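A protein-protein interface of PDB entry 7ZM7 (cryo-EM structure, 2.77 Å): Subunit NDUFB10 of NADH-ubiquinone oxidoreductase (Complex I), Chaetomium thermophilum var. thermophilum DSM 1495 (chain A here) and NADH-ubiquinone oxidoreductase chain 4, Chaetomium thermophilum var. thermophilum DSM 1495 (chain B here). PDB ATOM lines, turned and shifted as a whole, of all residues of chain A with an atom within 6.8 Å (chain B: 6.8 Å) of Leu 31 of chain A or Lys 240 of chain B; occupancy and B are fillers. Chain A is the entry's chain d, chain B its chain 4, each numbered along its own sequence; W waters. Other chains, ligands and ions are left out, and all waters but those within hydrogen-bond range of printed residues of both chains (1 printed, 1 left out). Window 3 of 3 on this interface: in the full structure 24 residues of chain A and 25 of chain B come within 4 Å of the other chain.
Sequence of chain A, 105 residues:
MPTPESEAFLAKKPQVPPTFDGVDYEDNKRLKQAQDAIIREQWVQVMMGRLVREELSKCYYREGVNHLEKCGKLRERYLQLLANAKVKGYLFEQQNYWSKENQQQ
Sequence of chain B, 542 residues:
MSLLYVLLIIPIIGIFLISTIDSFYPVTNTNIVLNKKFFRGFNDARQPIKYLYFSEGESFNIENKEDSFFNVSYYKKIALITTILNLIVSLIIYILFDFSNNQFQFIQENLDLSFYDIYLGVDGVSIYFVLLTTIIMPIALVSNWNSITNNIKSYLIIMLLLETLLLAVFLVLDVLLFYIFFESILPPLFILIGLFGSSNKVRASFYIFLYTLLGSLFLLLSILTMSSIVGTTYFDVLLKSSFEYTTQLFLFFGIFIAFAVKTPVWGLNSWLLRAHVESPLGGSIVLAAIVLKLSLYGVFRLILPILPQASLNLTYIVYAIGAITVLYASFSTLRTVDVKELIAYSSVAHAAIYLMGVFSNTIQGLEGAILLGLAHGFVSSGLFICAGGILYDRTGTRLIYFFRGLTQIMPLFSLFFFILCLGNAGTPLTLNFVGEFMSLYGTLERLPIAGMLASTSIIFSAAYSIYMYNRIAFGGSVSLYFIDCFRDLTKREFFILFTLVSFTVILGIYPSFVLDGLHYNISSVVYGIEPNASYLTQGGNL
O of Tyr 25 of chain A sits at hydrogen-bond distance from NZ of Lys 240 of chain B (3.0 Å).
O of Lys 32 of chain A lies within hydrogen-bond range of ND2 of Asn 102 of chain B (2.9 Å).
OE1 of Gln 35 of chain A lies within hydrogen-bond range of ND2 of Asn 102 of chain B (3.4 Å).
The side-chain hydroxyl (OG) of Ser 242 of chain B sits at hydrogen-bond distance from the side-chain amide oxygen (OE1) of Gln 95 of chain A, at 3.4 Å.
The backbone NH of Glu 26 of chain A sits at hydrogen-bond distance from the side-chain carboxylate of Asp 24 of chain A, at 3.2 Å.
The backbone carbonyl oxygen of Gln 94 of chain A lies within hydrogen-bond range of the side-chain hydroxyl of Tyr 25 of chain A (2.7 Å).
The side-chain amide oxygen (OE1) of Gln 94 of chain A lies within hydrogen-bond range of the side-chain amide nitrogen (NE2) of Gln 35 of chain A (2.6 Å).
Among the printed residues, pairs that only touch across the chains: Glu 26 of chain A with Lys 240 of chain B (3.3 Å), Asn 28 of chain A with Lys 240 of chain B (3.6 Å), Leu 31 of chain A with Lys 240 of chain B (3.8 Å), Asp 36 of chain A with Asn 102 of chain B (3.997 Å) and Gln 94 of chain A with Leu 239 of chain B (3.5 Å).
Of chain B, only Lys 240 comes within 4 Å of Leu 31 of chain A.
Of chain A, only Tyr 25, Glu 26, Asn 28 and Leu 31 come within 4 Å of Lys 240 of chain B.
Of the printed residues of chain A, Ser 242 of chain B touches Gln 95 (3.4 Å).
Of the printed residues of chain B, Glu 26 of chain A touches Lys 240.
Gln 33 of chain A touches none of the printed residues of chain B.
The nearest residue of chain B that does not touch Leu 31 of chain A is Asp 236 of chain B (5.7 Å).
Of the 10 printed residues of chain B, 4 touch a printed residue of chain A.
Of the 19 printed residues of chain A, 9 touch a printed residue of chain B.
Hydrophobic or aromatic side chains of chain A that line the printed part of chain B: Leu 31.
Among the printed residues, 9 pairs touch across the chains.
Among the printed residues, no Asp or Glu carboxylate lies within 4 Å of a Lys or Arg side-chain nitrogen of the other chain.
Water W1 lies within hydrogen-bond range of OD2 of Asp 36 of chain A (2.7 Å) and N of Asn 102 of chain B (3.0 Å).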
ATOM      1  N   THR A  19     -15.584 -19.074   7.581  1.00  0.00           N
ATOM      2  CA  THR A  19     -15.577 -17.939   8.484  1.00  0.00           C
ATOM      3  C   THR A  19     -16.078 -18.388   9.844  1.00  0.00           C
ATOM      4  O   THR A  19     -16.443 -19.544  10.051  1.00  0.00           O
ATOM      5  CB  THR A  19     -16.448 -16.803   7.954  1.00  0.00           C
ATOM      6  OG1 THR A  19     -16.281 -15.647   8.782  1.00  0.00           O
ATOM      7  CG2 THR A  19     -17.900 -17.215   7.959  1.00  0.00           C
ATOM      8  N   PHE A  20     -16.083 -17.455  10.774  1.00  0.00           N
ATOM      9  CA  PHE A  20     -16.708 -17.645  12.064  1.00  0.00           C
ATOM     10  C   PHE A  20     -17.708 -16.548  12.368  1.00  0.00           C
ATOM     11  O   PHE A  20     -18.389 -16.626  13.393  1.00  0.00           O
ATOM     12  CB  PHE A  20     -15.650 -17.710  13.168  1.00  0.00           C
ATOM     13  CG  PHE A  20     -14.873 -18.975  13.161  1.00  0.00           C
ATOM     14  CD1 PHE A  20     -15.443 -20.149  13.606  1.00  0.00           C
ATOM     15  CD2 PHE A  20     -13.594 -19.011  12.679  1.00  0.00           C
ATOM     16  CE1 PHE A  20     -14.737 -21.314  13.585  1.00  0.00           C
ATOM     17  CE2 PHE A  20     -12.900 -20.184  12.655  1.00  0.00           C
ATOM     18  CZ  PHE A  20     -13.475 -21.327  13.110  1.00  0.00           C
ATOM     19  N   VAL A  23     -21.434 -17.364  13.740  1.00  0.00           N
ATOM     20  CA  VAL A  23     -21.405 -18.804  13.973  1.00  0.00           C
ATOM     21  C   VAL A  23     -21.490 -19.037  15.470  1.00  0.00           C
ATOM     22  O   VAL A  23     -20.556 -18.700  16.207  1.00  0.00           O
ATOM     23  CB  VAL A  23     -20.139 -19.455  13.402  1.00  0.00           C
ATOM     24  CG1 VAL A  23     -20.105 -20.928  13.754  1.00  0.00           C
ATOM     25  CG2 VAL A  23     -20.063 -19.252  11.902  1.00  0.00           C
ATOM     26  N   ASP A  24     -22.599 -19.614  15.919  1.00  0.00           N
ATOM     27  CA  ASP A  24     -22.739 -19.947  17.328  1.00  0.00           C
ATOM     28  C   ASP A  24     -21.761 -21.049  17.688  1.00  0.00           C
ATOM     29  O   ASP A  24     -21.722 -22.093  17.034  1.00  0.00           O
ATOM     30  CB  ASP A  24     -24.163 -20.390  17.638  1.00  0.00           C
ATOM     31  CG  ASP A  24     -24.349 -20.749  19.090  1.00  0.00           C
ATOM     32  OD1 ASP A  24     -24.412 -19.825  19.923  1.00  0.00           O
ATOM     33  OD2 ASP A  24     -24.425 -21.953  19.401  1.00  0.00           O
ATOM     34  N   TYR A  25     -20.946 -20.807  18.712  1.00  0.00           N
ATOM     35  CA  TYR A  25     -19.930 -21.788  19.063  1.00  0.00           C
ATOM     36  C   TYR A  25     -20.518 -22.963  19.828  1.00  0.00           C
ATOM     37  O   TYR A  25     -20.056 -24.094  19.661  1.00  0.00           O
ATOM     38  CB  TYR A  25     -18.807 -21.131  19.860  1.00  0.00           C
ATOM     39  CG  TYR A  25     -17.833 -20.380  18.994  1.00  0.00           C
ATOM     40  CD1 TYR A  25     -18.177 -19.993  17.720  1.00  0.00           C
ATOM     41  CD2 TYR A  25     -16.586 -20.037  19.454  1.00  0.00           C
ATOM     42  CE1 TYR A  25     -17.310 -19.300  16.932  1.00  0.00           C
ATOM     43  CE2 TYR A  25     -15.709 -19.342  18.661  1.00  0.00           C
ATOM     44  CZ  TYR A  25     -16.079 -18.977  17.403  1.00  0.00           C
ATOM     45  OH  TYR A  25     -15.225 -18.287  16.595  1.00  0.00           O
ATOM     46  N   GLU A  26     -21.549 -22.733  20.631  1.00  0.00           N
ATOM     47  CA  GLU A  26     -22.192 -23.837  21.326  1.00  0.00           C
ATOM     48  C   GLU A  26     -22.922 -24.775  20.377  1.00  0.00           C
ATOM     49  O   GLU A  26     -23.321 -25.867  20.795  1.00  0.00           O
ATOM     50  CB  GLU A  26     -23.137 -23.289  22.381  1.00  0.00           C
ATOM     51  CG  GLU A  26     -22.415 -22.564  23.490  1.00  0.00           C
ATOM     52  CD  GLU A  26     -23.346 -22.080  24.567  1.00  0.00           C
ATOM     53  OE1 GLU A  26     -24.574 -22.223  24.394  1.00  0.00           O
ATOM     54  OE2 GLU A  26     -22.857 -21.548  25.583  1.00  0.00           O
ATOM     55  N   ASP A  27     -23.064 -24.363  19.108  1.00  0.00           N
ATOM     56  CA  ASP A  27     -23.589 -25.296  18.088  1.00  0.00           C
ATOM     57  C   ASP A  27     -22.335 -25.961  17.562  1.00  0.00           C
ATOM     58  O   ASP A  27     -21.683 -25.360  16.706  1.00  0.00           O
ATOM     59  CB  ASP A  27     -24.246 -24.563  16.922  1.00  0.00           C
ATOM     60  CG  ASP A  27     -24.893 -25.484  15.901  1.00  0.00           C
ATOM     61  OD1 ASP A  27     -24.854 -26.715  16.103  1.00  0.00           O
ATOM     62  OD2 ASP A  27     -25.435 -24.964  14.911  1.00  0.00           O
ATOM     63  N   ASN A  28     -22.066 -27.175  18.012  1.00  0.00           N
ATOM     64  CA  ASN A  28     -20.809 -27.864  17.659  1.00  0.00           C
ATOM     65  C   ASN A  28     -20.741 -28.217  16.178  1.00  0.00           C
ATOM     66  O   ASN A  28     -19.676 -28.043  15.602  1.00  0.00           O
ATOM     67  CB  ASN A  28     -20.614 -29.067  18.581  1.00  0.00           C
ATOM     68  CG  ASN A  28     -20.864 -28.741  20.037  1.00  0.00           C
ATOM     69  OD1 ASN A  28     -21.916 -29.069  20.574  1.00  0.00           O
ATOM     70  ND2 ASN A  28     -19.907 -28.093  20.680  1.00  0.00           N
ATOM     71  N   LYS A  29     -21.831 -28.706  15.583  1.00  0.00           N
ATOM     72  CA  LYS A  29     -21.751 -29.178  14.177  1.00  0.00           C
ATOM     73  C   LYS A  29     -21.388 -28.010  13.262  1.00  0.00           C
ATOM     74  O   LYS A  29     -20.509 -28.186  12.417  1.00  0.00           O
ATOM     75  CB  LYS A  29     -23.080 -29.806  13.764  1.00  0.00           C
ATOM     76  CG  LYS A  29     -23.145 -30.297  12.324  1.00  0.00           C
ATOM     77  CD  LYS A  29     -24.470 -30.932  11.963  1.00  0.00           C
ATOM     78  CE  LYS A  29     -24.527 -31.403  10.525  1.00  0.00           C
ATOM     79  NZ  LYS A  29     -25.834 -32.018  10.201  1.00  0.00           N
ATOM     80  N   ARG A  30     -22.018 -26.856  13.461  1.00  0.00           N
ATOM     81  CA  ARG A  30     -21.732 -25.649  12.655  1.00  0.00           C
ATOM     82  C   ARG A  30     -20.301 -25.197  12.910  1.00  0.00           C
ATOM     83  O   ARG A  30     -19.631 -24.827  11.942  1.00  0.00           O
ATOM     84  CB  ARG A  30     -22.750 -24.567  13.018  1.00  0.00           C
ATOM     85  CG  ARG A  30     -22.661 -23.301  12.180  1.00  0.00           C
ATOM     86  CD  ARG A  30     -22.881 -23.575  10.705  1.00  0.00           C
ATOM     87  NE  ARG A  30     -22.401 -22.476   9.882  1.00  0.00           N
ATOM     88  CZ  ARG A  30     -21.160 -22.371   9.424  1.00  0.00           C
ATOM     89  NH1 ARG A  30     -20.271 -23.307   9.708  1.00  0.00           N
ATOM     90  NH2 ARG A  30     -20.811 -21.337   8.680  1.00  0.00           N
ATOM     91  N   LEU A  31     -19.868 -25.217  14.166  1.00  0.00           N
ATOM     92  CA  LEU A  31     -18.508 -24.734  14.515  1.00  0.00           C
ATOM     93  C   LEU A  31     -17.452 -25.633  13.871  1.00  0.00           C
ATOM     94  O   LEU A  31     -16.488 -25.086  13.343  1.00  0.00           O
ATOM     95  CB  LEU A  31     -18.380 -24.721  16.038  1.00  0.00           C
ATOM     96  CG  LEU A  31     -16.944 -24.706  16.563  1.00  0.00           C
ATOM     97  CD1 LEU A  31     -16.497 -23.296  16.913  1.00  0.00           C
ATOM     98  CD2 LEU A  31     -16.784 -25.633  17.753  1.00  0.00           C
ATOM     99  N   LYS A  32     -17.649 -26.951  13.926  1.00  0.00           N
ATOM    100  CA  LYS A  32     -16.696 -27.941  13.376  1.00  0.00           C
ATOM    101  C   LYS A  32     -16.649 -27.798  11.862  1.00  0.00           C
ATOM    102  O   LYS A  32     -15.565 -27.957  11.292  1.00  0.00           O
ATOM    103  CB  LYS A  32     -17.063 -29.351  13.834  1.00  0.00           C
ATOM    104  CG  LYS A  32     -16.890 -29.615  15.322  1.00  0.00           C
ATOM    105  CD  LYS A  32     -15.461 -29.854  15.738  1.00  0.00           C
ATOM    106  CE  LYS A  32     -14.958 -31.215  15.315  1.00  0.00           C
ATOM    107  NZ  LYS A  32     -13.509 -31.373  15.578  1.00  0.00           N
ATOM    108  N   GLN A  33     -17.788 -27.499  11.253  1.00  0.00           N
ATOM    109  CA  GLN A  33     -17.868 -27.331   9.790  1.00  0.00           C
ATOM    110  C   GLN A  33     -17.227 -26.003   9.441  1.00  0.00           C
ATOM    111  O   GLN A  33     -16.534 -25.969   8.434  1.00  0.00           O
ATOM    112  CB  GLN A  33     -19.333 -27.226   9.396  1.00  0.00           C
ATOM    113  CG  GLN A  33     -20.084 -28.544   9.422  1.00  0.00           C
ATOM    114  CD  GLN A  33     -21.464 -28.379   8.837  1.00  0.00           C
ATOM    115  OE1 GLN A  33     -21.945 -27.268   8.647  1.00  0.00           O
ATOM    116  NE2 GLN A  33     -22.115 -29.492   8.545  1.00  0.00           N
ATOM    117  N   ALA A  34     -17.392 -24.976  10.258  1.00  0.00           N
ATOM    118  CA  ALA A  34     -16.602 -23.788   9.994  1.00  0.00           C
ATOM    119  C   ALA A  34     -15.127 -24.125   9.984  1.00  0.00           C
ATOM    120  O   ALA A  34     -14.435 -23.863   9.002  1.00  0.00           O
ATOM    121  CB  ALA A  34     -16.899 -22.717  11.037  1.00  0.00           C
ATOM    122  N   GLN A  35     -14.643 -24.773  11.050  1.00  0.00           N
ATOM    123  CA  GLN A  35     -13.227 -25.119  11.133  1.00  0.00           C
ATOM    124  C   GLN A  35     -12.787 -25.874   9.894  1.00  0.00           C
ATOM    125  O   GLN A  35     -11.765 -25.542   9.290  1.00  0.00           O
ATOM    126  CB  GLN A  35     -12.951 -25.962  12.374  1.00  0.00           C
ATOM    127  CG  GLN A  35     -13.155 -25.282  13.695  1.00  0.00           C
ATOM    128  CD  GLN A  35     -13.301 -26.277  14.810  1.00  0.00           C
ATOM    129  OE1 GLN A  35     -13.478 -27.455  14.565  1.00  0.00           O
ATOM    130  NE2 GLN A  35     -13.219 -25.815  16.036  1.00  0.00           N
ATOM    131  N   ASP A  36     -13.563 -26.877   9.489  1.00  0.00           N
ATOM    132  CA  ASP A  36     -13.234 -27.656   8.304  1.00  0.00           C
ATOM    133  C   ASP A  36     -13.228 -26.813   7.038  1.00  0.00           C
ATOM    134  O   ASP A  36     -12.469 -27.102   6.113  1.00  0.00           O
ATOM    135  CB  ASP A  36     -14.214 -28.810   8.168  1.00  0.00           C
ATOM    136  CG  ASP A  36     -13.901 -29.704   7.000  1.00  0.00           C
ATOM    137  OD1 ASP A  36     -14.141 -29.302   5.845  1.00  0.00           O
ATOM    138  OD2 ASP A  36     -13.436 -30.831   7.233  1.00  0.00           O
ATOM    139  N   ILE A  38     -12.340 -23.565   6.719  1.00  0.00           N
ATOM    140  CA  ILE A  38     -11.104 -22.795   6.632  1.00  0.00           C
ATOM    141  C   ILE A  38      -9.920 -23.693   6.295  1.00  0.00           C
ATOM    142  O   ILE A  38      -9.043 -23.306   5.518  1.00  0.00           O
ATOM    143  CB  ILE A  38     -10.869 -21.959   7.910  1.00  0.00           C
ATOM    144  CG1 ILE A  38     -11.955 -20.903   8.105  1.00  0.00           C
ATOM    145  CG2 ILE A  38      -9.542 -21.246   7.895  1.00  0.00           C
ATOM    146  CD1 ILE A  38     -13.124 -21.314   8.854  1.00  0.00           C
ATOM    147  N   GLN A  94     -10.558 -18.550  14.983  1.00  0.00           N
ATOM    148  CA  GLN A  94     -11.642 -18.955  15.870  1.00  0.00           C
ATOM    149  C   GLN A  94     -11.690 -18.092  17.117  1.00  0.00           C
ATOM    150  O   GLN A  94     -12.769 -17.817  17.640  1.00  0.00           O
ATOM    151  CB  GLN A  94     -11.496 -20.423  16.254  1.00  0.00           C
ATOM    152  CG  GLN A  94     -12.728 -21.001  16.894  1.00  0.00           C
ATOM    153  CD  GLN A  94     -12.616 -22.468  17.148  1.00  0.00           C
ATOM    154  OE1 GLN A  94     -12.841 -23.274  16.262  1.00  0.00           O
ATOM    155  NE2 GLN A  94     -12.279 -22.833  18.367  1.00  0.00           N
ATOM    156  N   GLN A  95     -10.534 -17.661  17.601  1.00  0.00           N
ATOM    157  CA  GLN A  95     -10.410 -16.999  18.887  1.00  0.00           C
ATOM    158  C   GLN A  95     -10.297 -15.497  18.789  1.00  0.00           C
ATOM    159  O   GLN A  95     -10.162 -14.845  19.823  1.00  0.00           O
ATOM    160  CB  GLN A  95      -9.190 -17.513  19.623  1.00  0.00           C
ATOM    161  CG  GLN A  95      -9.199 -18.957  19.954  1.00  0.00           C
ATOM    162  CD  GLN A  95      -7.900 -19.362  20.555  1.00  0.00           C
ATOM    163  OE1 GLN A  95      -7.021 -18.531  20.751  1.00  0.00           O
ATOM    164  NE2 GLN A  95      -7.751 -20.638  20.843  1.00  0.00           N
ATOM    165  N   ASN B 102     -12.498 -34.113  10.686  1.00  0.00           N
ATOM    166  CA  ASN B 102     -12.138 -33.251  11.848  1.00  0.00           C
ATOM    167  C   ASN B 102     -12.998 -33.610  13.051  1.00  0.00           C
ATOM    168  O   ASN B 102     -12.990 -32.846  14.016  1.00  0.00           O
ATOM    169  CB  ASN B 102     -12.164 -31.753  11.537  1.00  0.00           C
ATOM    170  CG  ASN B 102     -13.522 -31.101  11.683  1.00  0.00           C
ATOM    171  OD1 ASN B 102     -14.548 -31.693  11.364  1.00  0.00           O
ATOM    172  ND2 ASN B 102     -13.532 -29.864  12.145  1.00  0.00           N
ATOM    173  N   PHE B 235     -12.238 -32.843  25.431  1.00  0.00           N
ATOM    174  CA  PHE B 235     -11.473 -32.079  24.446  1.00  0.00           C
ATOM    175  C   PHE B 235     -12.338 -31.056  23.723  1.00  0.00           C
ATOM    176  O   PHE B 235     -11.957 -29.890  23.599  1.00  0.00           O
ATOM    177  CB  PHE B 235     -10.815 -33.008  23.418  1.00  0.00           C
ATOM    178  CG  PHE B 235      -9.675 -33.828  23.944  1.00  0.00           C
ATOM    179  CD1 PHE B 235      -8.968 -33.448  25.062  1.00  0.00           C
ATOM    180  CD2 PHE B 235      -9.280 -34.965  23.278  1.00  0.00           C
ATOM    181  CE1 PHE B 235      -7.905 -34.225  25.516  1.00  0.00           C
ATOM    182  CE2 PHE B 235      -8.232 -35.723  23.726  1.00  0.00           C
ATOM    183  CZ  PHE B 235      -7.550 -35.356  24.841  1.00  0.00           C
ATOM    184  N   ASP B 236     -13.507 -31.473  23.240  1.00  0.00           N
ATOM    185  CA  ASP B 236     -14.317 -30.603  22.393  1.00  0.00           C
ATOM    186  C   ASP B 236     -14.730 -29.318  23.087  1.00  0.00           C
ATOM    187  O   ASP B 236     -14.952 -28.311  22.415  1.00  0.00           O
ATOM    188  CB  ASP B 236     -15.554 -31.337  21.917  1.00  0.00           C
ATOM    189  CG  ASP B 236     -15.253 -32.313  20.823  1.00  0.00           C
ATOM    190  OD1 ASP B 236     -14.288 -32.074  20.069  1.00  0.00           O
ATOM    191  OD2 ASP B 236     -15.980 -33.323  20.709  1.00  0.00           O
ATOM    192  N   VAL B 237     -14.841 -29.322  24.408  1.00  0.00           N
ATOM    193  CA  VAL B 237     -15.240 -28.115  25.111  1.00  0.00           C
ATOM    194  C   VAL B 237     -14.033 -27.248  25.455  1.00  0.00           C
ATOM    195  O   VAL B 237     -14.151 -26.023  25.495  1.00  0.00           O
ATOM    196  CB  VAL B 237     -16.052 -28.494  26.362  1.00  0.00           C
ATOM    197  CG1 VAL B 237     -16.435 -27.263  27.166  1.00  0.00           C
ATOM    198  CG2 VAL B 237     -17.264 -29.303  25.992  1.00  0.00           C
ATOM    199  N   LEU B 238     -12.866 -27.859  25.692  1.00  0.00           N
ATOM    200  CA  LEU B 238     -11.627 -27.106  25.901  1.00  0.00           C
ATOM    201  C   LEU B 238     -11.142 -26.384  24.655  1.00  0.00           C
ATOM    202  O   LEU B 238     -10.642 -25.262  24.748  1.00  0.00           O
ATOM    203  CB  LEU B 238     -10.517 -28.020  26.409  1.00  0.00           C
ATOM    204  CG  LEU B 238     -10.592 -28.655  27.779  1.00  0.00           C
ATOM    205  CD1 LEU B 238      -9.456 -29.601  27.936  1.00  0.00           C
ATOM    206  CD2 LEU B 238     -10.393 -27.528  28.765  1.00  0.00           C
ATOM    207  N   LEU B 239     -11.192 -27.032  23.496  1.00  0.00           N
ATOM    208  CA  LEU B 239     -10.625 -26.406  22.308  1.00  0.00           C
ATOM    209  C   LEU B 239     -11.455 -25.207  21.862  1.00  0.00           C
ATOM    210  O   LEU B 239     -10.921 -24.259  21.277  1.00  0.00           O
ATOM    211  CB  LEU B 239     -10.499 -27.437  21.197  1.00  0.00           C
ATOM    212  CG  LEU B 239      -9.933 -28.785  21.626  1.00  0.00           C
ATOM    213  CD1 LEU B 239      -9.831 -29.712  20.419  1.00  0.00           C
ATOM    214  CD2 LEU B 239      -8.611 -28.691  22.385  1.00  0.00           C
ATOM    215  N   LYS B 240     -12.751 -25.231  22.145  1.00  0.00           N
ATOM    216  CA  LYS B 240     -13.577 -24.047  21.976  1.00  0.00           C
ATOM    217  C   LYS B 240     -13.088 -22.897  22.847  1.00  0.00           C
ATOM    218  O   LYS B 240     -13.047 -21.746  22.407  1.00  0.00           O
ATOM    219  CB  LYS B 240     -15.013 -24.396  22.329  1.00  0.00           C
ATOM    220  CG  LYS B 240     -15.682 -25.307  21.369  1.00  0.00           C
ATOM    221  CD  LYS B 240     -17.016 -25.676  21.934  1.00  0.00           C
ATOM    222  CE  LYS B 240     -17.962 -24.528  21.925  1.00  0.00           C
ATOM    223  NZ  LYS B 240     -19.283 -24.993  22.393  1.00  0.00           N
ATOM    224  N   SER B 241     -12.786 -23.205  24.099  1.00  0.00           N
ATOM    225  CA  SER B 241     -12.478 -22.144  25.085  1.00  0.00           C
ATOM    226  C   SER B 241     -11.101 -21.506  24.912  1.00  0.00           C
ATOM    227  O   SER B 241     -10.129 -22.246  24.717  1.00  0.00           O
ATOM    228  CB  SER B 241     -12.654 -22.716  26.454  1.00  0.00           C
ATOM    229  OG  SER B 241     -14.003 -23.111  26.657  1.00  0.00           O
ATOM    230  N   SER B 242     -11.035 -20.180  24.995  1.00  0.00           N
ATOM    231  CA  SER B 242      -9.724 -19.496  24.951  1.00  0.00           C
ATOM    232  C   SER B 242      -9.408 -18.834  26.298  1.00  0.00           C
ATOM    233  O   SER B 242     -10.085 -17.865  26.661  1.00  0.00           O
ATOM    234  CB  SER B 242      -9.665 -18.526  23.826  1.00  0.00           C
ATOM    235  OG  SER B 242      -8.418 -17.845  23.814  1.00  0.00           O
ATOM    236  N   ILE B 306      -4.877 -25.062  23.257  1.00  0.00           N
ATOM    237  CA  ILE B 306      -5.541 -24.307  24.311  1.00  0.00           C
ATOM    238  C   ILE B 306      -4.668 -23.243  24.967  1.00  0.00           C
ATOM    239  O   ILE B 306      -5.216 -22.356  25.633  1.00  0.00           O
ATOM    240  CB  ILE B 306      -6.136 -25.242  25.382  1.00  0.00           C
ATOM    241  CG1 ILE B 306      -5.048 -26.047  26.051  1.00  0.00           C
ATOM    242  CG2 ILE B 306      -7.179 -26.151  24.795  1.00  0.00           C
ATOM    243  CD1 ILE B 306      -5.532 -26.779  27.215  1.00  0.00           C
HETATM  244  O   HOH W   1     -13.916 -33.290   8.161  1.00  0.00           O
